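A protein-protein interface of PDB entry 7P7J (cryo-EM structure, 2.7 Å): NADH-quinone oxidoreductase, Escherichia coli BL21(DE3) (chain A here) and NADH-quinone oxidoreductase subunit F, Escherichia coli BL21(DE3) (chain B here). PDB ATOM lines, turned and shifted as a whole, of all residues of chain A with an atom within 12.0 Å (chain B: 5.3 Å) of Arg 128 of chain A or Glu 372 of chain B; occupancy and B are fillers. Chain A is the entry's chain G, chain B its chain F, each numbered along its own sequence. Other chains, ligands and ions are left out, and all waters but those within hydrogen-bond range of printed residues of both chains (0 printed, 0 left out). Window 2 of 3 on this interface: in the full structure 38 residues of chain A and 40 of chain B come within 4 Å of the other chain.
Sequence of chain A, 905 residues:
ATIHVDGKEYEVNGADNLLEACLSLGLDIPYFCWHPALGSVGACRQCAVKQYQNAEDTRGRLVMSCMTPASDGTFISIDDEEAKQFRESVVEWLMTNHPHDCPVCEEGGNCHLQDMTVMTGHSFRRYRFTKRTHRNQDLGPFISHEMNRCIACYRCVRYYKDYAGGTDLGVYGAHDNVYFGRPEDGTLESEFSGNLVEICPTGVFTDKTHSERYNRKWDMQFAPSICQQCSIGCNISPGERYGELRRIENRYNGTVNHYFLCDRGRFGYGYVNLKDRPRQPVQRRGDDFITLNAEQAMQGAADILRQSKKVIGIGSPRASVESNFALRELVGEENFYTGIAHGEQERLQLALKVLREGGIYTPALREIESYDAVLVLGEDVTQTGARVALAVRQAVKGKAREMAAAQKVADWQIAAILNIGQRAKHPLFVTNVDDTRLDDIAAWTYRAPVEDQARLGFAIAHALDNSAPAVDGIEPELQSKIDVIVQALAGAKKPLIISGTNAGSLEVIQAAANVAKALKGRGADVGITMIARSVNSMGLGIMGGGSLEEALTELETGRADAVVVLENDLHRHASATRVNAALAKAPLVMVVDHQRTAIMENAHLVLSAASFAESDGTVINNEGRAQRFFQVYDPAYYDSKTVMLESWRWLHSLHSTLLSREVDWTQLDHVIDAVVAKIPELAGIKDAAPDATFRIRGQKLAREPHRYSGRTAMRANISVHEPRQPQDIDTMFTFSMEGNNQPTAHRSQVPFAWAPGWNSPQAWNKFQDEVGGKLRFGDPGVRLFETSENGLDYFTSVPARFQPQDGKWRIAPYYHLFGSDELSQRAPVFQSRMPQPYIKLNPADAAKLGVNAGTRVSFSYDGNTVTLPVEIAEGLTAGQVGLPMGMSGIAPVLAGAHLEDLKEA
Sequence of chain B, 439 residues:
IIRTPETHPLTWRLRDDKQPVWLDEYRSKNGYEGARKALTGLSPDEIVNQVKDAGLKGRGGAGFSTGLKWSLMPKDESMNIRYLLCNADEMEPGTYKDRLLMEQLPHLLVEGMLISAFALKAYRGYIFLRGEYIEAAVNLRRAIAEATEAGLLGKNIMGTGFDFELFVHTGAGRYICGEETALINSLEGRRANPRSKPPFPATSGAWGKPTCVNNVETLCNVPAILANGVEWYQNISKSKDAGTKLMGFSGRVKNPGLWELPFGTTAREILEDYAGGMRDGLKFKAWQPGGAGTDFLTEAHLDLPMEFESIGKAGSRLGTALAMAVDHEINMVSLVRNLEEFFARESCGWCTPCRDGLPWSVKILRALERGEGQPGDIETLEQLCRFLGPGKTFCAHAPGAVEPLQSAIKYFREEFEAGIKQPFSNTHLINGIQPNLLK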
ATOM      1  N   GLU A  92      24.210 -11.047  -2.217  1.00  0.00           N
ATOM      2  CA  GLU A  92      24.239  -9.868  -3.076  1.00  0.00           C
ATOM      3  C   GLU A  92      24.829  -8.660  -2.358  1.00  0.00           C
ATOM      4  O   GLU A  92      25.608  -7.907  -2.949  1.00  0.00           O
ATOM      5  CB  GLU A  92      22.830  -9.562  -3.571  1.00  0.00           C
ATOM      6  CG  GLU A  92      22.732  -8.332  -4.432  1.00  0.00           C
ATOM      7  CD  GLU A  92      21.345  -8.126  -4.984  1.00  0.00           C
ATOM      8  OE1 GLU A  92      20.367  -8.387  -4.257  1.00  0.00           O
ATOM      9  OE2 GLU A  92      21.229  -7.705  -6.151  1.00  0.00           O
ATOM     10  N   TRP A  93      24.470  -8.463  -1.086  1.00  0.00           N
ATOM     11  CA  TRP A  93      25.026  -7.361  -0.305  1.00  0.00           C
ATOM     12  C   TRP A  93      26.520  -7.532  -0.098  1.00  0.00           C
ATOM     13  O   TRP A  93      27.267  -6.549  -0.076  1.00  0.00           O
ATOM     14  CB  TRP A  93      24.329  -7.255   1.048  1.00  0.00           C
ATOM     15  CG  TRP A  93      22.944  -6.733   0.981  1.00  0.00           C
ATOM     16  CD1 TRP A  93      22.477  -5.748   0.169  1.00  0.00           C
ATOM     17  CD2 TRP A  93      21.834  -7.165   1.767  1.00  0.00           C
ATOM     18  NE1 TRP A  93      21.142  -5.543   0.396  1.00  0.00           N
ATOM     19  CE2 TRP A  93      20.724  -6.401   1.376  1.00  0.00           C
ATOM     20  CE3 TRP A  93      21.673  -8.126   2.766  1.00  0.00           C
ATOM     21  CZ2 TRP A  93      19.469  -6.570   1.944  1.00  0.00           C
ATOM     22  CZ3 TRP A  93      20.429  -8.295   3.324  1.00  0.00           C
ATOM     23  CH2 TRP A  93      19.343  -7.519   2.917  1.00  0.00           C
ATOM     24  N   MET A  95      28.311  -8.957  -2.307  1.00  0.00           N
ATOM     25  CA  MET A  95      28.843  -8.818  -3.653  1.00  0.00           C
ATOM     26  C   MET A  95      28.876  -7.378  -4.145  1.00  0.00           C
ATOM     27  O   MET A  95      29.430  -7.129  -5.219  1.00  0.00           O
ATOM     28  CB  MET A  95      28.013  -9.673  -4.609  1.00  0.00           C
ATOM     29  CG  MET A  95      28.617 -11.028  -4.883  1.00  0.00           C
ATOM     30  SD  MET A  95      30.388 -10.942  -5.092  1.00  0.00           S
ATOM     31  CE  MET A  95      30.864 -12.096  -3.834  1.00  0.00           C
ATOM     32  N   THR A  96      28.298  -6.434  -3.401  1.00  0.00           N
ATOM     33  CA  THR A  96      28.243  -5.053  -3.870  1.00  0.00           C
ATOM     34  C   THR A  96      29.605  -4.380  -3.831  1.00  0.00           C
ATOM     35  O   THR A  96      29.888  -3.514  -4.664  1.00  0.00           O
ATOM     36  CB  THR A  96      27.248  -4.242  -3.042  1.00  0.00           C
ATOM     37  OG1 THR A  96      27.532  -4.413  -1.651  1.00  0.00           O
ATOM     38  CG2 THR A  96      25.828  -4.680  -3.325  1.00  0.00           C
ATOM     39  N   ASN A  97      30.450  -4.743  -2.871  1.00  0.00           N
ATOM     40  CA  ASN A  97      31.763  -4.134  -2.720  1.00  0.00           C
ATOM     41  C   ASN A  97      32.888  -5.078  -3.109  1.00  0.00           C
ATOM     42  O   ASN A  97      34.060  -4.741  -2.918  1.00  0.00           O
ATOM     43  CB  ASN A  97      31.958  -3.660  -1.283  1.00  0.00           C
ATOM     44  CG  ASN A  97      31.031  -2.530  -0.915  1.00  0.00           C
ATOM     45  OD1 ASN A  97      30.990  -1.504  -1.586  1.00  0.00           O
ATOM     46  ND2 ASN A  97      30.277  -2.712   0.159  1.00  0.00           N
ATOM     47  N   HIS A  98      32.567  -6.233  -3.646  1.00  0.00           N
ATOM     48  CA  HIS A  98      33.615  -7.206  -3.885  1.00  0.00           C
ATOM     49  C   HIS A  98      34.375  -6.876  -5.167  1.00  0.00           C
ATOM     50  O   HIS A  98      33.760  -6.543  -6.182  1.00  0.00           O
ATOM     51  CB  HIS A  98      33.037  -8.609  -3.972  1.00  0.00           C
ATOM     52  CG  HIS A  98      34.048  -9.674  -3.716  1.00  0.00           C
ATOM     53  ND1 HIS A  98      34.649  -9.838  -2.490  1.00  0.00           N
ATOM     54  CD2 HIS A  98      34.596 -10.600  -4.533  1.00  0.00           C
ATOM     55  CE1 HIS A  98      35.518 -10.827  -2.560  1.00  0.00           C
ATOM     56  NE2 HIS A  98      35.502 -11.308  -3.788  1.00  0.00           N
ATOM     57  N   HIS A 122      22.730 -16.603  -7.121  1.00  0.00           N
ATOM     58  CA  HIS A 122      22.804 -15.175  -7.390  1.00  0.00           C
ATOM     59  C   HIS A 122      23.868 -14.929  -8.451  1.00  0.00           C
ATOM     60  O   HIS A 122      25.061 -15.114  -8.197  1.00  0.00           O
ATOM     61  CB  HIS A 122      23.113 -14.393  -6.117  1.00  0.00           C
ATOM     62  CG  HIS A 122      23.223 -12.921  -6.339  1.00  0.00           C
ATOM     63  ND1 HIS A 122      22.143 -12.142  -6.690  1.00  0.00           N
ATOM     64  CD2 HIS A 122      24.287 -12.089  -6.290  1.00  0.00           C
ATOM     65  CE1 HIS A 122      22.537 -10.891  -6.840  1.00  0.00           C
ATOM     66  NE2 HIS A 122      23.834 -10.832  -6.603  1.00  0.00           N
ATOM     67  N   PHE A 124      23.060 -12.220 -11.141  1.00  0.00           N
ATOM     68  CA  PHE A 124      22.715 -10.983 -11.825  1.00  0.00           C
ATOM     69  C   PHE A 124      22.962  -9.816 -10.882  1.00  0.00           C
ATOM     70  O   PHE A 124      22.445  -9.800  -9.761  1.00  0.00           O
ATOM     71  CB  PHE A 124      21.257 -11.001 -12.286  1.00  0.00           C
ATOM     72  CG  PHE A 124      20.894  -9.872 -13.200  1.00  0.00           C
ATOM     73  CD1 PHE A 124      21.095  -9.980 -14.564  1.00  0.00           C
ATOM     74  CD2 PHE A 124      20.342  -8.705 -12.699  1.00  0.00           C
ATOM     75  CE1 PHE A 124      20.762  -8.945 -15.407  1.00  0.00           C
ATOM     76  CE2 PHE A 124      20.009  -7.666 -13.537  1.00  0.00           C
ATOM     77  CZ  PHE A 124      20.219  -7.787 -14.893  1.00  0.00           C
ATOM     78  N   ARG A 125      23.736  -8.841 -11.341  1.00  0.00           N
ATOM     79  CA  ARG A 125      24.120  -7.692 -10.535  1.00  0.00           C
ATOM     80  C   ARG A 125      23.215  -6.517 -10.873  1.00  0.00           C
ATOM     81  O   ARG A 125      23.165  -6.084 -12.027  1.00  0.00           O
ATOM     82  CB  ARG A 125      25.582  -7.330 -10.787  1.00  0.00           C
ATOM     83  CG  ARG A 125      26.102  -6.160  -9.976  1.00  0.00           C
ATOM     84  CD  ARG A 125      27.569  -5.918 -10.274  1.00  0.00           C
ATOM     85  NE  ARG A 125      28.176  -4.933  -9.390  1.00  0.00           N
ATOM     86  CZ  ARG A 125      28.627  -5.195  -8.172  1.00  0.00           C
ATOM     87  NH1 ARG A 125      28.511  -6.398  -7.637  1.00  0.00           N
ATOM     88  NH2 ARG A 125      29.213  -4.227  -7.475  1.00  0.00           N
ATOM     89  N   ARG A 126      22.507  -6.002  -9.870  1.00  0.00           N
ATOM     90  CA  ARG A 126      21.697  -4.802 -10.027  1.00  0.00           C
ATOM     91  C   ARG A 126      22.245  -3.634  -9.216  1.00  0.00           C
ATOM     92  O   ARG A 126      21.538  -2.646  -8.999  1.00  0.00           O
ATOM     93  CB  ARG A 126      20.241  -5.082  -9.656  1.00  0.00           C
ATOM     94  CG  ARG A 126      20.028  -5.503  -8.224  1.00  0.00           C
ATOM     95  CD  ARG A 126      18.686  -6.192  -8.044  1.00  0.00           C
ATOM     96  NE  ARG A 126      17.936  -5.617  -6.936  1.00  0.00           N
ATOM     97  CZ  ARG A 126      17.771  -6.199  -5.755  1.00  0.00           C
ATOM     98  NH1 ARG A 126      18.269  -7.396  -5.499  1.00  0.00           N
ATOM     99  NH2 ARG A 126      17.084  -5.565  -4.811  1.00  0.00           N
ATOM    100  N   TYR A 127      23.491  -3.726  -8.772  1.00  0.00           N
ATOM    101  CA  TYR A 127      24.164  -2.650  -8.060  1.00  0.00           C
ATOM    102  C   TYR A 127      25.058  -1.912  -9.047  1.00  0.00           C
ATOM    103  O   TYR A 127      25.923  -2.523  -9.681  1.00  0.00           O
ATOM    104  CB  TYR A 127      24.974  -3.215  -6.893  1.00  0.00           C
ATOM    105  CG  TYR A 127      25.696  -2.197  -6.040  1.00  0.00           C
ATOM    106  CD1 TYR A 127      25.059  -1.565  -4.986  1.00  0.00           C
ATOM    107  CD2 TYR A 127      27.027  -1.897  -6.272  1.00  0.00           C
ATOM    108  CE1 TYR A 127      25.722  -0.651  -4.201  1.00  0.00           C
ATOM    109  CE2 TYR A 127      27.695  -0.984  -5.493  1.00  0.00           C
ATOM    110  CZ  TYR A 127      27.040  -0.366  -4.459  1.00  0.00           C
ATOM    111  OH  TYR A 127      27.716   0.544  -3.685  1.00  0.00           O
ATOM    112  N   ARG A 128      24.851  -0.603  -9.175  1.00  0.00           N
ATOM    113  CA  ARG A 128      25.537   0.195 -10.183  1.00  0.00           C
ATOM    114  C   ARG A 128      26.466   1.244  -9.589  1.00  0.00           C
ATOM    115  O   ARG A 128      27.012   2.064 -10.336  1.00  0.00           O
ATOM    116  CB  ARG A 128      24.516   0.880 -11.091  1.00  0.00           C
ATOM    117  CG  ARG A 128      23.727   1.963 -10.391  1.00  0.00           C
ATOM    118  CD  ARG A 128      22.813   2.685 -11.347  1.00  0.00           C
ATOM    119  NE  ARG A 128      22.013   3.698 -10.670  1.00  0.00           N
ATOM    120  CZ  ARG A 128      20.891   3.446 -10.013  1.00  0.00           C
ATOM    121  NH1 ARG A 128      20.404   2.221  -9.923  1.00  0.00           N
ATOM    122  NH2 ARG A 128      20.244   4.447  -9.427  1.00  0.00           N
ATOM    123  N   PHE A 129      26.669   1.244  -8.285  1.00  0.00           N
ATOM    124  CA  PHE A 129      27.415   2.299  -7.629  1.00  0.00           C
ATOM    125  C   PHE A 129      28.875   1.890  -7.458  1.00  0.00           C
ATOM    126  O   PHE A 129      29.331   0.877  -7.993  1.00  0.00           O
ATOM    127  CB  PHE A 129      26.742   2.639  -6.303  1.00  0.00           C
ATOM    128  CG  PHE A 129      25.299   3.009  -6.445  1.00  0.00           C
ATOM    129  CD1 PHE A 129      24.937   4.237  -6.963  1.00  0.00           C
ATOM    130  CD2 PHE A 129      24.304   2.127  -6.069  1.00  0.00           C
ATOM    131  CE1 PHE A 129      23.610   4.580  -7.099  1.00  0.00           C
ATOM    132  CE2 PHE A 129      22.975   2.465  -6.202  1.00  0.00           C
ATOM    133  CZ  PHE A 129      22.629   3.695  -6.720  1.00  0.00           C
ATOM    134  N   THR A 130      29.626   2.694  -6.716  1.00  0.00           N
ATOM    135  CA  THR A 130      31.035   2.412  -6.510  1.00  0.00           C
ATOM    136  C   THR A 130      31.223   1.384  -5.400  1.00  0.00           C
ATOM    137  O   THR A 130      30.361   1.183  -4.544  1.00  0.00           O
ATOM    138  CB  THR A 130      31.804   3.686  -6.172  1.00  0.00           C
ATOM    139  OG1 THR A 130      31.310   4.235  -4.946  1.00  0.00           O
ATOM    140  CG2 THR A 130      31.646   4.709  -7.280  1.00  0.00           C
ATOM    141  N   LYS A 131      32.376   0.729  -5.430  1.00  0.00           N
ATOM    142  CA  LYS A 131      32.748  -0.267  -4.440  1.00  0.00           C
ATOM    143  C   LYS A 131      33.889   0.274  -3.594  1.00  0.00           C
ATOM    144  O   LYS A 131      34.787   0.946  -4.108  1.00  0.00           O
ATOM    145  CB  LYS A 131      33.163  -1.574  -5.112  1.00  0.00           C
ATOM    146  CG  LYS A 131      32.301  -1.944  -6.301  1.00  0.00           C
ATOM    147  CD  LYS A 131      32.607  -3.336  -6.809  1.00  0.00           C
ATOM    148  CE  LYS A 131      33.942  -3.383  -7.506  1.00  0.00           C
ATOM    149  NZ  LYS A 131      34.118  -4.657  -8.242  1.00  0.00           N
ATOM    150  N   ARG A 132      33.841  -0.002  -2.296  1.00  0.00           N
ATOM    151  CA  ARG A 132      34.888   0.464  -1.402  1.00  0.00           C
ATOM    152  C   ARG A 132      36.178  -0.307  -1.646  1.00  0.00           C
ATOM    153  O   ARG A 132      36.168  -1.469  -2.058  1.00  0.00           O
ATOM    154  CB  ARG A 132      34.448   0.328   0.056  1.00  0.00           C
ATOM    155  CG  ARG A 132      34.088  -1.079   0.494  1.00  0.00           C
ATOM    156  CD  ARG A 132      35.211  -1.729   1.283  1.00  0.00           C
ATOM    157  NE  ARG A 132      34.954  -3.138   1.550  1.00  0.00           N
ATOM    158  CZ  ARG A 132      35.486  -4.140   0.864  1.00  0.00           C
ATOM    159  NH1 ARG A 132      36.265  -3.924  -0.182  1.00  0.00           N
ATOM    160  NH2 ARG A 132      35.219  -5.388   1.230  1.00  0.00           N
ATOM    161  N   ALA B 367      21.092   9.206  -5.371  1.00  0.00           N
ATOM    162  CA  ALA B 367      20.735   9.264  -6.784  1.00  0.00           C
ATOM    163  C   ALA B 367      19.349   9.862  -6.984  1.00  0.00           C
ATOM    164  O   ALA B 367      19.124  10.614  -7.938  1.00  0.00           O
ATOM    165  CB  ALA B 367      20.816   7.870  -7.401  1.00  0.00           C
ATOM    166  N   LEU B 368      18.404   9.529  -6.104  1.00  0.00           N
ATOM    167  CA  LEU B 368      17.066  10.110  -6.194  1.00  0.00           C
ATOM    168  C   LEU B 368      17.078  11.597  -5.871  1.00  0.00           C
ATOM    169  O   LEU B 368      16.248  12.350  -6.393  1.00  0.00           O
ATOM    170  CB  LEU B 368      16.100   9.383  -5.259  1.00  0.00           C
ATOM    171  CG  LEU B 368      15.737   7.942  -5.613  1.00  0.00           C
ATOM    172  CD1 LEU B 368      14.782   7.366  -4.592  1.00  0.00           C
ATOM    173  CD2 LEU B 368      15.146   7.859  -7.001  1.00  0.00           C
ATOM    174  N   ARG B 370      19.538  13.710  -6.646  1.00  0.00           N
ATOM    175  CA  ARG B 370      20.091  14.386  -7.810  1.00  0.00           C
ATOM    176  C   ARG B 370      19.309  14.105  -9.084  1.00  0.00           C
ATOM    177  O   ARG B 370      19.714  14.567 -10.155  1.00  0.00           O
ATOM    178  CB  ARG B 370      21.553  13.980  -8.014  1.00  0.00           C
ATOM    179  CG  ARG B 370      22.415  14.102  -6.772  1.00  0.00           C
ATOM    180  CD  ARG B 370      23.871  13.819  -7.090  1.00  0.00           C
ATOM    181  NE  ARG B 370      24.038  12.555  -7.797  1.00  0.00           N
ATOM    182  CZ  ARG B 370      24.348  11.405  -7.215  1.00  0.00           C
ATOM    183  NH1 ARG B 370      24.541  11.320  -5.909  1.00  0.00           N
ATOM    184  NH2 ARG B 370      24.469  10.311  -7.962  1.00  0.00           N
ATOM    185  N   GLY B 371      18.213  13.357  -9.001  1.00  0.00           N
ATOM    186  CA  GLY B 371      17.452  13.008 -10.179  1.00  0.00           C
ATOM    187  C   GLY B 371      18.061  11.919 -11.027  1.00  0.00           C
ATOM    188  O   GLY B 371      17.579  11.677 -12.138  1.00  0.00           O
ATOM    189  N   GLU B 372      19.109  11.253 -10.542  1.00  0.00           N
ATOM    190  CA  GLU B 372      19.771  10.181 -11.274  1.00  0.00           C
ATOM    191  C   GLU B 372      19.223   8.808 -10.921  1.00  0.00           C
ATOM    192  O   GLU B 372      19.940   7.807 -11.047  1.00  0.00           O
ATOM    193  CB  GLU B 372      21.277  10.232 -11.024  1.00  0.00           C
ATOM    194  CG  GLU B 372      21.907  11.573 -11.335  1.00  0.00           C
ATOM    195  CD  GLU B 372      23.359  11.641 -10.913  1.00  0.00           C
ATOM    196  OE1 GLU B 372      23.841  10.677 -10.281  1.00  0.00           O
ATOM    197  OE2 GLU B 372      24.020  12.657 -11.213  1.00  0.00           O
ATOM    198  N   GLY B 373      17.974   8.733 -10.469  1.00  0.00           N
ATOM    199  CA  GLY B 373      17.389   7.449 -10.152  1.00  0.00           C
ATOM    200  C   GLY B 373      17.092   6.639 -11.399  1.00  0.00           C
ATOM    201  O   GLY B 373      16.901   7.171 -12.490  1.00  0.00           O
ATOM    202  N   GLN B 374      17.056   5.329 -11.224  1.00  0.00           N
ATOM    203  CA  GLN B 374      16.839   4.371 -12.295  1.00  0.00           C
ATOM    204  C   GLN B 374      15.751   3.403 -11.862  1.00  0.00           C
ATOM    205  O   GLN B 374      15.495   3.254 -10.663  1.00  0.00           O
ATOM    206  CB  GLN B 374      18.143   3.627 -12.621  1.00  0.00           C
ATOM    207  CG  GLN B 374      19.180   4.523 -13.270  1.00  0.00           C
ATOM    208  CD  GLN B 374      20.422   3.782 -13.696  1.00  0.00           C
ATOM    209  OE1 GLN B 374      20.470   2.556 -13.663  1.00  0.00           O
ATOM    210  NE2 GLN B 374      21.443   4.527 -14.093  1.00  0.00           N
ATOM    211  N   ASP B 377      14.906   1.076  -8.329  1.00  0.00           N
ATOM    212  CA  ASP B 377      15.506   1.649  -7.127  1.00  0.00           C
ATOM    213  C   ASP B 377      14.530   1.651  -5.958  1.00  0.00           C
ATOM    214  O   ASP B 377      14.910   1.325  -4.828  1.00  0.00           O
ATOM    215  CB  ASP B 377      16.004   3.065  -7.413  1.00  0.00           C
ATOM    216  CG  ASP B 377      17.427   3.086  -7.938  1.00  0.00           C
ATOM    217  OD1 ASP B 377      18.127   2.061  -7.804  1.00  0.00           O
ATOM    218  OD2 ASP B 377      17.850   4.128  -8.477  1.00  0.00           O
ATOM    219  N   GLY B 419      12.327  11.102  -8.598  1.00  0.00           N
ATOM    220  CA  GLY B 419      13.770  11.130  -8.716  1.00  0.00           C
ATOM    221  C   GLY B 419      14.289  10.178  -9.771  1.00  0.00           C
ATOM    222  O   GLY B 419      15.482  10.175 -10.079  1.00  0.00           O
ATOM    223  N   LYS B 421      14.761   9.416 -13.307  1.00  0.00           N
ATOM    224  CA  LYS B 421      14.772  10.078 -14.605  1.00  0.00           C
ATOM    225  C   LYS B 421      15.615   9.381 -15.658  1.00  0.00           C
ATOM    226  O   LYS B 421      15.456   9.692 -16.844  1.00  0.00           O
ATOM    227  CB  LYS B 421      15.270  11.525 -14.469  1.00  0.00           C
ATOM    228  CG  LYS B 421      14.487  12.379 -13.487  1.00  0.00           C
ATOM    229  CD  LYS B 421      13.021  12.458 -13.868  1.00  0.00           C
ATOM    230  CE  LYS B 421      12.295  13.490 -13.025  1.00  0.00           C
ATOM    231  NZ  LYS B 421      10.817  13.420 -13.194  1.00  0.00           N
ATOM    232  N   GLN B 422      16.499   8.462 -15.282  1.00  0.00           N
ATOM    233  CA  GLN B 422      17.369   7.797 -16.233  1.00  0.00           C
ATOM    234  C   GLN B 422      16.965   6.337 -16.409  1.00  0.00           C
ATOM    235  O   GLN B 422      16.470   5.711 -15.469  1.00  0.00           O
ATOM    236  CB  GLN B 422      18.831   7.861 -15.775  1.00  0.00           C
ATOM    237  CG  GLN B 422      19.131   9.008 -14.836  1.00  0.00           C
ATOM    238  CD  GLN B 422      20.602   9.363 -14.807  1.00  0.00           C
ATOM    239  OE1 GLN B 422      21.456   8.503 -14.592  1.00  0.00           O
ATOM    240  NE2 GLN B 422      20.908  10.636 -15.025  1.00  0.00           N
ATOM    241  N   PHE B 424      17.618   2.272 -16.754  1.00  0.00           N
ATOM    242  CA  PHE B 424      18.534   1.411 -16.020  1.00  0.00           C
ATOM    243  C   PHE B 424      19.720   1.020 -16.889  1.00  0.00           C
ATOM    244  O   PHE B 424      19.553   0.558 -18.021  1.00  0.00           O
ATOM    245  CB  PHE B 424      17.826   0.157 -15.518  1.00  0.00           C
ATOM    246  CG  PHE B 424      18.723  -0.755 -14.732  1.00  0.00           C
ATOM    247  CD1 PHE B 424      19.130  -0.412 -13.452  1.00  0.00           C
ATOM    248  CD2 PHE B 424      19.176  -1.945 -15.277  1.00  0.00           C
ATOM    249  CE1 PHE B 424      19.963  -1.243 -12.728  1.00  0.00           C
ATOM    250  CE2 PHE B 424      20.010  -2.780 -14.555  1.00  0.00           C
ATOM    251  CZ  PHE B 424      20.401  -2.427 -13.279  1.00  0.00           C
ATOM    252  N   SER B 425      20.920   1.203 -16.349  1.00  0.00           N
ATOM    253  CA  SER B 425      22.145   0.873 -17.070  1.00  0.00           C
ATOM    254  C   SER B 425      23.170   0.407 -16.049  1.00  0.00           C
ATOM    255  O   SER B 425      23.696   1.215 -15.280  1.00  0.00           O
ATOM    256  CB  SER B 425      22.663   2.069 -17.861  1.00  0.00           C
ATOM    257  OG  SER B 425      23.865   1.744 -18.534  1.00  0.00           O
ATOM    258  N   ASN B 426      23.435  -0.896 -16.035  1.00  0.00           N
ATOM    259  CA  ASN B 426      24.473  -1.468 -15.198  1.00  0.00           C
ATOM    260  C   ASN B 426      25.714  -1.868 -15.980  1.00  0.00           C
ATOM    261  O   ASN B 426      26.788  -1.985 -15.384  1.00  0.00           O
ATOM    262  CB  ASN B 426      23.932  -2.697 -14.454  1.00  0.00           C
ATOM    263  CG  ASN B 426      24.634  -2.936 -13.144  1.00  0.00           C
ATOM    264  OD1 ASN B 426      25.332  -2.064 -12.636  1.00  0.00           O
ATOM    265  ND2 ASN B 426      24.457  -4.123 -12.588  1.00  0.00           N
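Of the printed residues of chain B, Arg 125 of chain A touches Asn 426 (2.4 Å). Of the printed residues of chain B, Arg 126 of chain A touches Asn 426. Of the printed residues of chain B, Tyr 127 of chain A touches Asn 426 (3.0 Å). Of the printed residues of chain B, Arg 128 of chain A touches Glu 372 (3.7 Å), Gln 374 (3.3 Å), Asp 377 (2.6 Å) and Asn 426 (3.3 Å). No residue of chain A comes within 4 Å of Leu 368 of chain B. Arg 370 of chain B touches none of the printed residues of chain A. Gly 371 of chain B touches none of the printed residues of chain A. Of the printed residues of chain A, Glu 372 of chain B touches Arg 128. Gln 374 of chain B touches just one residue of chain A: Arg 128 (3.3 Å). No residue of chain A comes within 4 Å of Gln 422 of chain B. No residue of chain A comes within 4 Å of Phe 424 of chain B. No residue of chain A comes within 4 Å of Ser 425 of chain B. Asn 426 of chain B touches just these residues of chain A: Arg 125, Arg 126, Tyr 127 and Arg 128. The nearest printed residue of chain B that does not touch Arg 128 of chain A is Ala 367 of chain B (4.02 Å). The nearest printed residue of chain B that does not touch Arg 125 of chain A is Phe 424 of chain B (4.8 Å).
Of the 14 printed residues of chain B, 4 touch a printed residue of chain A. Printed residues of chain B that touch a printed residue of chain A: Glu 372, Gln 374, Asp 377 and Asn 426. Of the 16 printed residues of chain A, 4 touch a printed residue of chain B. Among the printed residues, Asp or Glu carboxylates within 4 Å of a Lys or Arg side-chain nitrogen of the other chain: Arg 128 of chain A with Asp 377 of chain B.
CA of Arg 126 of chain A touches ND2 of Asn 426 of chain B, 3.8 Å away. O of Glu 372 of chain B touches NH2 of Arg 128 of chain A, at 3.7 Å. Arg 128 of chain A touches Gln 374 of chain B. Asn 426 of chain B touches Arg 128 of chain A (OD1 to CA, 3.3 Å).
OD1 of Asn 426 of chain B lies close to O of Tyr 127 of chain A (3.0 Å). NH2 of Arg 128 of chain A lies within salt-bridge range of OD2 of Asp 377 of chain B (2.6 Å). The side-chain amide nitrogen (ND2) of Asn 426 of chain B sits at hydrogen-bond distance from the backbone carbonyl oxygen (O) of Arg 125 of chain A (2.4 Å).
NE of Arg 125 of chain A sits at hydrogen-bond distance from O of Tyr 127 of chain A. N of Gln 374 of chain B is in hydrogen-bond range of OD2 of Asp 377 of chain B (3.1 Å). OE1 of Glu 372 of chain B lies within salt-bridge range of NH2 of Arg 370 of chain B. The side-chain carboxylate (OE1) of Glu 92 of chain A is in salt-bridge range of the guanidinium group (NH1) of Arg 126 of chain A. NH2 of Arg 125 of chain A is in hydrogen-bond range of O of Thr 96 of chain A, at 3.0 Å. The side-chain hydroxyl (OH) of Tyr 127 of chain A sits at hydrogen-bond distance from the backbone carbonyl oxygen (O) of Thr 130 of chain A (2.9 Å).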
